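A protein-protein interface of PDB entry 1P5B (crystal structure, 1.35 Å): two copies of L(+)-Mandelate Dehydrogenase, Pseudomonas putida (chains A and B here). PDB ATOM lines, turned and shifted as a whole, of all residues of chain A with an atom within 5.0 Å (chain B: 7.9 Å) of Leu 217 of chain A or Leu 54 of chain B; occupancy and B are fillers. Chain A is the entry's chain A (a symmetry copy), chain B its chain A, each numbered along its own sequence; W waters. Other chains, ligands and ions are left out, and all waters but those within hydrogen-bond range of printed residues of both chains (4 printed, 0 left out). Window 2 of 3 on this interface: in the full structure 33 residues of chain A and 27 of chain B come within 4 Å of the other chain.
O of Leu 54 of chain B sits at hydrogen-bond distance from N of Trp 214 of chain A, 3.3 Å away.
Printed residues of chain A that touch a printed residue of chain B: Thr 157, Phe 212, Asn 213, Trp 214 and Leu 217.
Printed residues of chain B that touch a printed residue of chain A: Arg 53 and Leu 54.
Among the printed residues, 7 pairs touch across the chains.
Leu 217 of chain A touches just one residue of chain B: Leu 54.
Of chain A, only Thr 157 (3.9 Å), Phe 212 (3.7 Å), Asn 213 (3.0 Å), Trp 214 (3.3 Å) and Leu 217 (3.7 Å) come within 4 Å of Leu 54 of chain B.
Of the printed residues of chain B, Thr 157 of chain A touches Arg 53 and Leu 54.
Of the printed residues of chain A, Arg 53 of chain B touches Thr 157 (3.5 Å) and Trp 214 (3.5 Å).
Glu 245 of chain A touches none of the printed residues of chain B.
The nearest printed residue of chain B that does not touch Leu 217 of chain A is Arg 53 of chain B (8.2 Å).
The nearest printed residue of chain B that does not touch Thr 157 of chain A is Lys 52 of chain B (6.8 Å).
Arg 53 of chain B touches Thr 157 of chain A (CD to OG1, 3.5 Å).
Thr 157 of chain A touches Leu 54 of chain B.
Leu 54 of chain B touches Phe 212 of chain A (CD2 to O, 3.7 Å).
Asn 213 of chain A touches Leu 54 of chain B.
Trp 214 of chain A touches Arg 53 of chain B (CZ2 to O, 3.5 Å).
Leu 54 of chain B touches Leu 217 of chain A (CD1 to CD2, 3.7 Å).
The side-chain amide oxygen (OD1) of Asn 213 of chain A sits close to the backbone NH (N) of Glu 215 of chain A, at 3.2 Å.
OD1 of Asn 213 of chain A sits at hydrogen-bond distance from N of Ala 216 of chain A.
Water W3 bridges the backbone carbonyl oxygen of Phe 212 of chain A (2.7 Å) and the backbone carbonyl oxygen of Val 55 of chain B (3.0 Å).
Water W2 bridges the backbone carbonyl oxygen of Thr 157 of chain A and the backbone NH of Leu 54 of chain B.
Water W1 bridges the backbone NH of Asp 56 of chain B and the side-chain amide nitrogen of Asn 213 of chain A.
Water W4 lies within hydrogen-bond range of the guanidinium group (NH1) of Arg 53 of chain B (2.8 Å) and the backbone carbonyl oxygen (O) of Thr 157 of chain A (3.3 Å).
No position is printed for both chains.
Of the 7 pairs that touch across the chains among the printed residues, none has its exchanged pair printed and touching as well.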
ATOM      1  N   LEU A 155       7.366 -17.386  -1.476  1.00  0.00           N
ATOM      2  CA  LEU A 155       7.265 -16.097  -2.144  1.00  0.00           C
ATOM      3  C   LEU A 155       8.415 -15.227  -1.657  1.00  0.00           C
ATOM      4  O   LEU A 155       8.531 -14.970  -0.459  1.00  0.00           O
ATOM      5  CB  LEU A 155       5.944 -15.401  -1.806  1.00  0.00           C
ATOM      6  CG  LEU A 155       5.835 -13.970  -2.342  1.00  0.00           C
ATOM      7  CD1 LEU A 155       5.726 -13.996  -3.860  1.00  0.00           C
ATOM      8  CD2 LEU A 155       4.626 -13.274  -1.727  1.00  0.00           C
ATOM      9  N   THR A 157       9.957 -11.749  -1.266  1.00  0.00           N
ATOM     10  CA  THR A 157       9.473 -10.379  -1.240  1.00  0.00           C
ATOM     11  C   THR A 157      10.508  -9.270  -1.145  1.00  0.00           C
ATOM     12  O   THR A 157      10.134  -8.096  -1.095  1.00  0.00           O
ATOM     13  CB  THR A 157       8.521 -10.194  -0.051  1.00  0.00           C
ATOM     14  OG1 THR A 157       9.259 -10.352   1.171  1.00  0.00           O
ATOM     15  CG2 THR A 157       7.406 -11.237  -0.092  1.00  0.00           C
ATOM     16  N   PHE A 212       3.118  -5.627  -5.437  1.00  0.00           N
ATOM     17  CA  PHE A 212       2.695  -6.820  -4.711  1.00  0.00           C
ATOM     18  C   PHE A 212       2.697  -6.560  -3.211  1.00  0.00           C
ATOM     19  O   PHE A 212       3.753  -6.396  -2.596  1.00  0.00           O
ATOM     20  CB  PHE A 212       3.606  -8.003  -5.056  1.00  0.00           C
ATOM     21  CG  PHE A 212       2.949  -9.343  -4.873  1.00  0.00           C
ATOM     22  CD1 PHE A 212       2.868  -9.934  -3.617  1.00  0.00           C
ATOM     23  CD2 PHE A 212       2.376  -9.999  -5.960  1.00  0.00           C
ATOM     24  CE1 PHE A 212       2.223 -11.160  -3.444  1.00  0.00           C
ATOM     25  CE2 PHE A 212       1.729 -11.222  -5.797  1.00  0.00           C
ATOM     26  CZ  PHE A 212       1.652 -11.803  -4.537  1.00  0.00           C
ATOM     27  N   ASN A 213       1.503  -6.521  -2.627  1.00  0.00           N
ATOM     28  CA  ASN A 213       1.349  -6.247  -1.204  1.00  0.00           C
ATOM     29  C   ASN A 213       0.581  -7.334  -0.462  1.00  0.00           C
ATOM     30  O   ASN A 213       0.385  -8.434  -0.973  1.00  0.00           O
ATOM     31  CB  ASN A 213       0.639  -4.906  -1.012  1.00  0.00           C
ATOM     32  CG  ASN A 213      -0.659  -4.823  -1.788  1.00  0.00           C
ATOM     33  OD1 ASN A 213      -1.226  -5.843  -2.178  1.00  0.00           O
ATOM     34  ND2 ASN A 213      -1.142  -3.606  -2.006  1.00  0.00           N
ATOM     35  N   TRP A 214       0.144  -7.011   0.749  1.00  0.00           N
ATOM     36  CA  TRP A 214      -0.592  -7.959   1.572  1.00  0.00           C
ATOM     37  C   TRP A 214      -1.842  -8.486   0.881  1.00  0.00           C
ATOM     38  O   TRP A 214      -2.159  -9.671   0.988  1.00  0.00           O
ATOM     39  CB  TRP A 214      -0.954  -7.319   2.912  1.00  0.00           C
ATOM     40  CG  TRP A 214       0.255  -6.938   3.707  1.00  0.00           C
ATOM     41  CD1 TRP A 214       0.713  -5.676   3.949  1.00  0.00           C
ATOM     42  CD2 TRP A 214       1.185  -7.830   4.330  1.00  0.00           C
ATOM     43  NE1 TRP A 214       1.874  -5.726   4.685  1.00  0.00           N
ATOM     44  CE2 TRP A 214       2.186  -7.038   4.932  1.00  0.00           C
ATOM     45  CE3 TRP A 214       1.271  -9.225   4.435  1.00  0.00           C
ATOM     46  CZ2 TRP A 214       3.261  -7.594   5.634  1.00  0.00           C
ATOM     47  CZ3 TRP A 214       2.340  -9.776   5.134  1.00  0.00           C
ATOM     48  CH2 TRP A 214       3.322  -8.959   5.723  1.00  0.00           C
ATOM     49  N   GLU A 215      -2.548  -7.608   0.173  1.00  0.00           N
ATOM     50  CA  GLU A 215      -3.752  -8.007  -0.545  1.00  0.00           C
ATOM     51  C   GLU A 215      -3.391  -9.056  -1.592  1.00  0.00           C
ATOM     52  O   GLU A 215      -4.101 -10.048  -1.770  1.00  0.00           O
ATOM     53  CB  GLU A 215      -4.387  -6.794  -1.229  1.00  0.00           C
ATOM     54  CG  GLU A 215      -5.587  -7.132  -2.095  1.00  0.00           C
ATOM     55  CD  GLU A 215      -6.164  -5.914  -2.787  1.00  0.00           C
ATOM     56  OE1 GLU A 215      -5.416  -5.241  -3.526  1.00  0.00           O
ATOM     57  OE2 GLU A 215      -7.366  -5.632  -2.593  1.00  0.00           O
ATOM     58  N   ALA A 216      -2.277  -8.830  -2.281  1.00  0.00           N
ATOM     59  CA  ALA A 216      -1.804  -9.754  -3.304  1.00  0.00           C
ATOM     60  C   ALA A 216      -1.385 -11.084  -2.682  1.00  0.00           C
ATOM     61  O   ALA A 216      -1.513 -12.137  -3.307  1.00  0.00           O
ATOM     62  CB  ALA A 216      -0.638  -9.138  -4.066  1.00  0.00           C
ATOM     63  N   LEU A 217      -0.871 -11.040  -1.454  1.00  0.00           N
ATOM     64  CA  LEU A 217      -0.466 -12.265  -0.774  1.00  0.00           C
ATOM     65  C   LEU A 217      -1.710 -13.113  -0.515  1.00  0.00           C
ATOM     66  O   LEU A 217      -1.661 -14.337  -0.591  1.00  0.00           O
ATOM     67  CB  LEU A 217       0.238 -11.949   0.551  1.00  0.00           C
ATOM     68  CG  LEU A 217       0.621 -13.160   1.412  1.00  0.00           C
ATOM     69  CD1 LEU A 217       1.546 -14.093   0.640  1.00  0.00           C
ATOM     70  CD2 LEU A 217       1.294 -12.681   2.686  1.00  0.00           C
ATOM     71  N   ARG A 218      -2.822 -12.452  -0.208  1.00  0.00           N
ATOM     72  CA  ARG A 218      -4.079 -13.149   0.046  1.00  0.00           C
ATOM     73  C   ARG A 218      -4.486 -13.902  -1.217  1.00  0.00           C
ATOM     74  O   ARG A 218      -4.971 -15.033  -1.157  1.00  0.00           O
ATOM     75  CB  ARG A 218      -5.163 -12.142   0.441  1.00  0.00           C
ATOM     76  CG  ARG A 218      -4.847 -11.393   1.728  1.00  0.00           C
ATOM     77  CD  ARG A 218      -5.788 -10.220   1.957  1.00  0.00           C
ATOM     78  NE  ARG A 218      -5.423  -9.472   3.158  1.00  0.00           N
ATOM     79  CZ  ARG A 218      -5.909  -8.277   3.474  1.00  0.00           C
ATOM     80  NH1 ARG A 218      -6.787  -7.682   2.676  1.00  0.00           N
ATOM     81  NH2 ARG A 218      -5.519  -7.675   4.590  1.00  0.00           N
ATOM     82  N   TRP A 219      -4.278 -13.262  -2.363  1.00  0.00           N
ATOM     83  CA  TRP A 219      -4.596 -13.867  -3.649  1.00  0.00           C
ATOM     84  C   TRP A 219      -3.749 -15.125  -3.844  1.00  0.00           C
ATOM     85  O   TRP A 219      -4.258 -16.177  -4.229  1.00  0.00           O
ATOM     86  CB  TRP A 219      -4.311 -12.870  -4.775  1.00  0.00           C
ATOM     87  CG  TRP A 219      -4.231 -13.500  -6.126  1.00  0.00           C
ATOM     88  CD1 TRP A 219      -5.268 -13.985  -6.871  1.00  0.00           C
ATOM     89  CD2 TRP A 219      -3.042 -13.743  -6.885  1.00  0.00           C
ATOM     90  NE1 TRP A 219      -4.797 -14.516  -8.048  1.00  0.00           N
ATOM     91  CE2 TRP A 219      -3.433 -14.381  -8.081  1.00  0.00           C
ATOM     92  CE3 TRP A 219      -1.681 -13.484  -6.667  1.00  0.00           C
ATOM     93  CZ2 TRP A 219      -2.512 -14.763  -9.062  1.00  0.00           C
ATOM     94  CZ3 TRP A 219      -0.765 -13.866  -7.641  1.00  0.00           C
ATOM     95  CH2 TRP A 219      -1.187 -14.500  -8.825  1.00  0.00           C
ATOM     96  N   LEU A 220      -2.454 -15.011  -3.570  1.00  0.00           N
ATOM     97  CA  LEU A 220      -1.547 -16.142  -3.721  1.00  0.00           C
ATOM     98  C   LEU A 220      -1.909 -17.274  -2.763  1.00  0.00           C
ATOM     99  O   LEU A 220      -1.814 -18.449  -3.116  1.00  0.00           O
ATOM    100  CB  LEU A 220      -0.101 -15.698  -3.474  1.00  0.00           C
ATOM    101  CG  LEU A 220       0.965 -16.777  -3.674  1.00  0.00           C
ATOM    102  CD1 LEU A 220       0.946 -17.270  -5.116  1.00  0.00           C
ATOM    103  CD2 LEU A 220       2.335 -16.205  -3.332  1.00  0.00           C
ATOM    104  N   ARG A 221      -2.318 -16.913  -1.550  1.00  0.00           N
ATOM    105  CA  ARG A 221      -2.698 -17.891  -0.535  1.00  0.00           C
ATOM    106  C   ARG A 221      -3.875 -18.742  -1.006  1.00  0.00           C
ATOM    107  O   ARG A 221      -3.930 -19.938  -0.732  1.00  0.00           O
ATOM    108  CB  ARG A 221      -3.066 -17.169   0.768  1.00  0.00           C
ATOM    109  CG  ARG A 221      -3.675 -18.051   1.864  1.00  0.00           C
ATOM    110  CD  ARG A 221      -2.681 -19.030   2.482  1.00  0.00           C
ATOM    111  NE  ARG A 221      -2.411 -20.194   1.639  1.00  0.00           N
ATOM    112  CZ  ARG A 221      -1.641 -21.215   2.004  1.00  0.00           C
ATOM    113  NH1 ARG A 221      -1.059 -21.219   3.199  1.00  0.00           N
ATOM    114  NH2 ARG A 221      -1.453 -22.239   1.183  1.00  0.00           N
ATOM    115  N   LEU A 228       2.852 -22.698   2.335  1.00  0.00           N
ATOM    116  CA  LEU A 228       3.267 -21.426   1.760  1.00  0.00           C
ATOM    117  C   LEU A 228       4.144 -20.647   2.733  1.00  0.00           C
ATOM    118  O   LEU A 228       3.751 -20.409   3.873  1.00  0.00           O
ATOM    119  CB  LEU A 228       2.034 -20.584   1.414  1.00  0.00           C
ATOM    120  CG  LEU A 228       2.276 -19.146   0.951  1.00  0.00           C
ATOM    121  CD1 LEU A 228       3.023 -19.148  -0.370  1.00  0.00           C
ATOM    122  CD2 LEU A 228       0.943 -18.427   0.809  1.00  0.00           C
ATOM    123  N   VAL A 230       6.751 -17.119   3.259  1.00  0.00           N
ATOM    124  CA  VAL A 230       7.102 -15.806   2.737  1.00  0.00           C
ATOM    125  C   VAL A 230       8.562 -15.591   3.127  1.00  0.00           C
ATOM    126  O   VAL A 230       8.926 -15.689   4.301  1.00  0.00           O
ATOM    127  CB  VAL A 230       6.222 -14.695   3.331  1.00  0.00           C
ATOM    128  CG1 VAL A 230       6.620 -13.353   2.742  1.00  0.00           C
ATOM    129  CG2 VAL A 230       4.754 -14.982   3.024  1.00  0.00           C
ATOM    130  N   CYS A 242       2.429 -12.117   8.208  1.00  0.00           N
ATOM    131  CA  CYS A 242       2.396 -13.166   7.196  1.00  0.00           C
ATOM    132  C   CYS A 242       1.574 -14.345   7.693  1.00  0.00           C
ATOM    133  O   CYS A 242       0.786 -14.919   6.940  1.00  0.00           O
ATOM    134  CB  CYS A 242       3.806 -13.639   6.856  1.00  0.00           C
ATOM    135  SG  CYS A 242       4.720 -12.513   5.794  1.00  0.00           S
ATOM    136  N   GLU A 245      -1.995 -13.538   7.657  1.00  0.00           N
ATOM    137  CA  GLU A 245      -2.525 -13.521   6.295  1.00  0.00           C
ATOM    138  C   GLU A 245      -2.620 -14.904   5.655  1.00  0.00           C
ATOM    139  O   GLU A 245      -2.978 -15.022   4.483  1.00  0.00           O
ATOM    140  CB  GLU A 245      -1.682 -12.607   5.401  1.00  0.00           C
ATOM    141  CG  GLU A 245      -1.707 -11.127   5.773  1.00  0.00           C
ATOM    142  CD  GLU A 245      -3.077 -10.486   5.610  1.00  0.00           C
ATOM    143  OE1 GLU A 245      -3.939 -11.071   4.922  1.00  0.00           O
ATOM    144  OE2 GLU A 245      -3.286  -9.384   6.162  1.00  0.00           O
ATOM    145  N   PRO B  51      13.324  -3.331   6.957  1.00  0.00           N
ATOM    146  CA  PRO B  51      12.346  -3.110   5.892  1.00  0.00           C
ATOM    147  C   PRO B  51      10.955  -3.613   6.230  1.00  0.00           C
ATOM    148  O   PRO B  51      10.788  -4.553   7.012  1.00  0.00           O
ATOM    149  CB  PRO B  51      12.934  -3.884   4.717  1.00  0.00           C
ATOM    150  CG  PRO B  51      14.407  -3.777   4.947  1.00  0.00           C
ATOM    151  CD  PRO B  51      14.525  -4.008   6.434  1.00  0.00           C
ATOM    152  N   LYS B  52       9.961  -2.961   5.639  1.00  0.00           N
ATOM    153  CA  LYS B  52       8.569  -3.353   5.792  1.00  0.00           C
ATOM    154  C   LYS B  52       8.249  -3.986   4.444  1.00  0.00           C
ATOM    155  O   LYS B  52       8.271  -3.315   3.409  1.00  0.00           O
ATOM    156  CB  LYS B  52       7.688  -2.132   6.048  1.00  0.00           C
ATOM    157  CG  LYS B  52       8.014  -1.434   7.361  1.00  0.00           C
ATOM    158  CD  LYS B  52       7.039  -0.315   7.668  1.00  0.00           C
ATOM    159  CE  LYS B  52       7.450   0.428   8.930  1.00  0.00           C
ATOM    160  NZ  LYS B  52       7.580  -0.484  10.098  1.00  0.00           N
ATOM    161  N   ARG B  53       7.982  -5.288   4.459  1.00  0.00           N
ATOM    162  CA  ARG B  53       7.702  -6.036   3.240  1.00  0.00           C
ATOM    163  C   ARG B  53       6.247  -6.001   2.807  1.00  0.00           C
ATOM    164  O   ARG B  53       5.364  -5.639   3.577  1.00  0.00           O
ATOM    165  CB  ARG B  53       8.137  -7.494   3.412  1.00  0.00           C
ATOM    166  CG  ARG B  53       9.632  -7.678   3.623  1.00  0.00           C
ATOM    167  CD  ARG B  53      10.423  -7.264   2.397  1.00  0.00           C
ATOM    168  NE  ARG B  53      11.858  -7.341   2.640  1.00  0.00           N
ATOM    169  CZ  ARG B  53      12.734  -6.436   2.220  1.00  0.00           C
ATOM    170  NH1 ARG B  53      12.326  -5.381   1.527  1.00  0.00           N
ATOM    171  NH2 ARG B  53      14.018  -6.578   2.510  1.00  0.00           N
ATOM    172  N   LEU B  54       6.022  -6.395   1.559  1.00  0.00           N
ATOM    173  CA  LEU B  54       4.691  -6.447   0.973  1.00  0.00           C
ATOM    174  C   LEU B  54       3.945  -5.124   1.016  1.00  0.00           C
ATOM    175  O   LEU B  54       2.732  -5.072   1.243  1.00  0.00           O
ATOM    176  CB  LEU B  54       3.882  -7.572   1.629  1.00  0.00           C
ATOM    177  CG  LEU B  54       4.431  -8.947   1.220  1.00  0.00           C
ATOM    178  CD1 LEU B  54       3.822 -10.044   2.069  1.00  0.00           C
ATOM    179  CD2 LEU B  54       4.143  -9.186  -0.252  1.00  0.00           C
ATOM    180  N   VAL B  55       4.698  -4.050   0.802  1.00  0.00           N
ATOM    181  CA  VAL B  55       4.145  -2.708   0.738  1.00  0.00           C
ATOM    182  C   VAL B  55       4.215  -2.332  -0.735  1.00  0.00           C
ATOM    183  O   VAL B  55       5.216  -2.597  -1.402  1.00  0.00           O
ATOM    184  CB  VAL B  55       4.986  -1.691   1.541  1.00  0.00           C
ATOM    185  CG1 VAL B  55       4.465  -0.275   1.303  1.00  0.00           C
ATOM    186  CG2 VAL B  55       4.934  -2.026   3.019  1.00  0.00           C
ATOM    187  N   ASP B  56       3.144  -1.742  -1.248  1.00  0.00           N
ATOM    188  CA  ASP B  56       3.110  -1.320  -2.640  1.00  0.00           C
ATOM    189  C   ASP B  56       4.071  -0.148  -2.814  1.00  0.00           C
ATOM    190  O   ASP B  56       3.795   0.957  -2.353  1.00  0.00           O
ATOM    191  CB  ASP B  56       1.687  -0.893  -3.016  1.00  0.00           C
ATOM    192  CG  ASP B  56       1.575  -0.402  -4.449  1.00  0.00           C
ATOM    193  OD1 ASP B  56       2.609  -0.285  -5.138  1.00  0.00           O
ATOM    194  OD2 ASP B  56       0.437  -0.124  -4.886  1.00  0.00           O
ATOM    195  N   VAL B  57       5.208  -0.395  -3.457  1.00  0.00           N
ATOM    196  CA  VAL B  57       6.181   0.667  -3.686  1.00  0.00           C
ATOM    197  C   VAL B  57       6.349   0.928  -5.180  1.00  0.00           C
ATOM    198  O   VAL B  57       7.402   1.372  -5.631  1.00  0.00           O
ATOM    199  CB  VAL B  57       7.564   0.329  -3.053  1.00  0.00           C
ATOM    200  CG1 VAL B  57       7.431   0.242  -1.540  1.00  0.00           C
ATOM    201  CG2 VAL B  57       8.107  -0.973  -3.612  1.00  0.00           C
ATOM    202  N   ALA B 338      12.261   2.139  -1.699  1.00  0.00           N
ATOM    203  CA  ALA B 338      11.546   0.983  -2.221  1.00  0.00           C
ATOM    204  C   ALA B 338      11.909  -0.250  -1.409  1.00  0.00           C
ATOM    205  O   ALA B 338      11.036  -1.019  -1.002  1.00  0.00           O
ATOM    206  CB  ALA B 338      11.903   0.763  -3.686  1.00  0.00           C
ATOM    207  N   GLY B 341      10.404  -0.356   2.091  1.00  0.00           N
ATOM    208  CA  GLY B 341       8.952  -0.293   2.112  1.00  0.00           C
ATOM    209  C   GLY B 341       8.332   1.026   2.524  1.00  0.00           C
ATOM    210  O   GLY B 341       7.266   1.047   3.140  1.00  0.00           O
HETATM  211  O   HOH W   1       0.654  -1.572   0.009  1.00  0.00           O
HETATM  212  O   HOH W   2       7.812  -6.627  -0.685  1.00  0.00           O
HETATM  213  O   HOH W   3       6.160  -5.191  -2.482  1.00  0.00           O
HETATM  214  O   HOH W   4      10.059  -4.991  -0.133  1.00  0.00           O
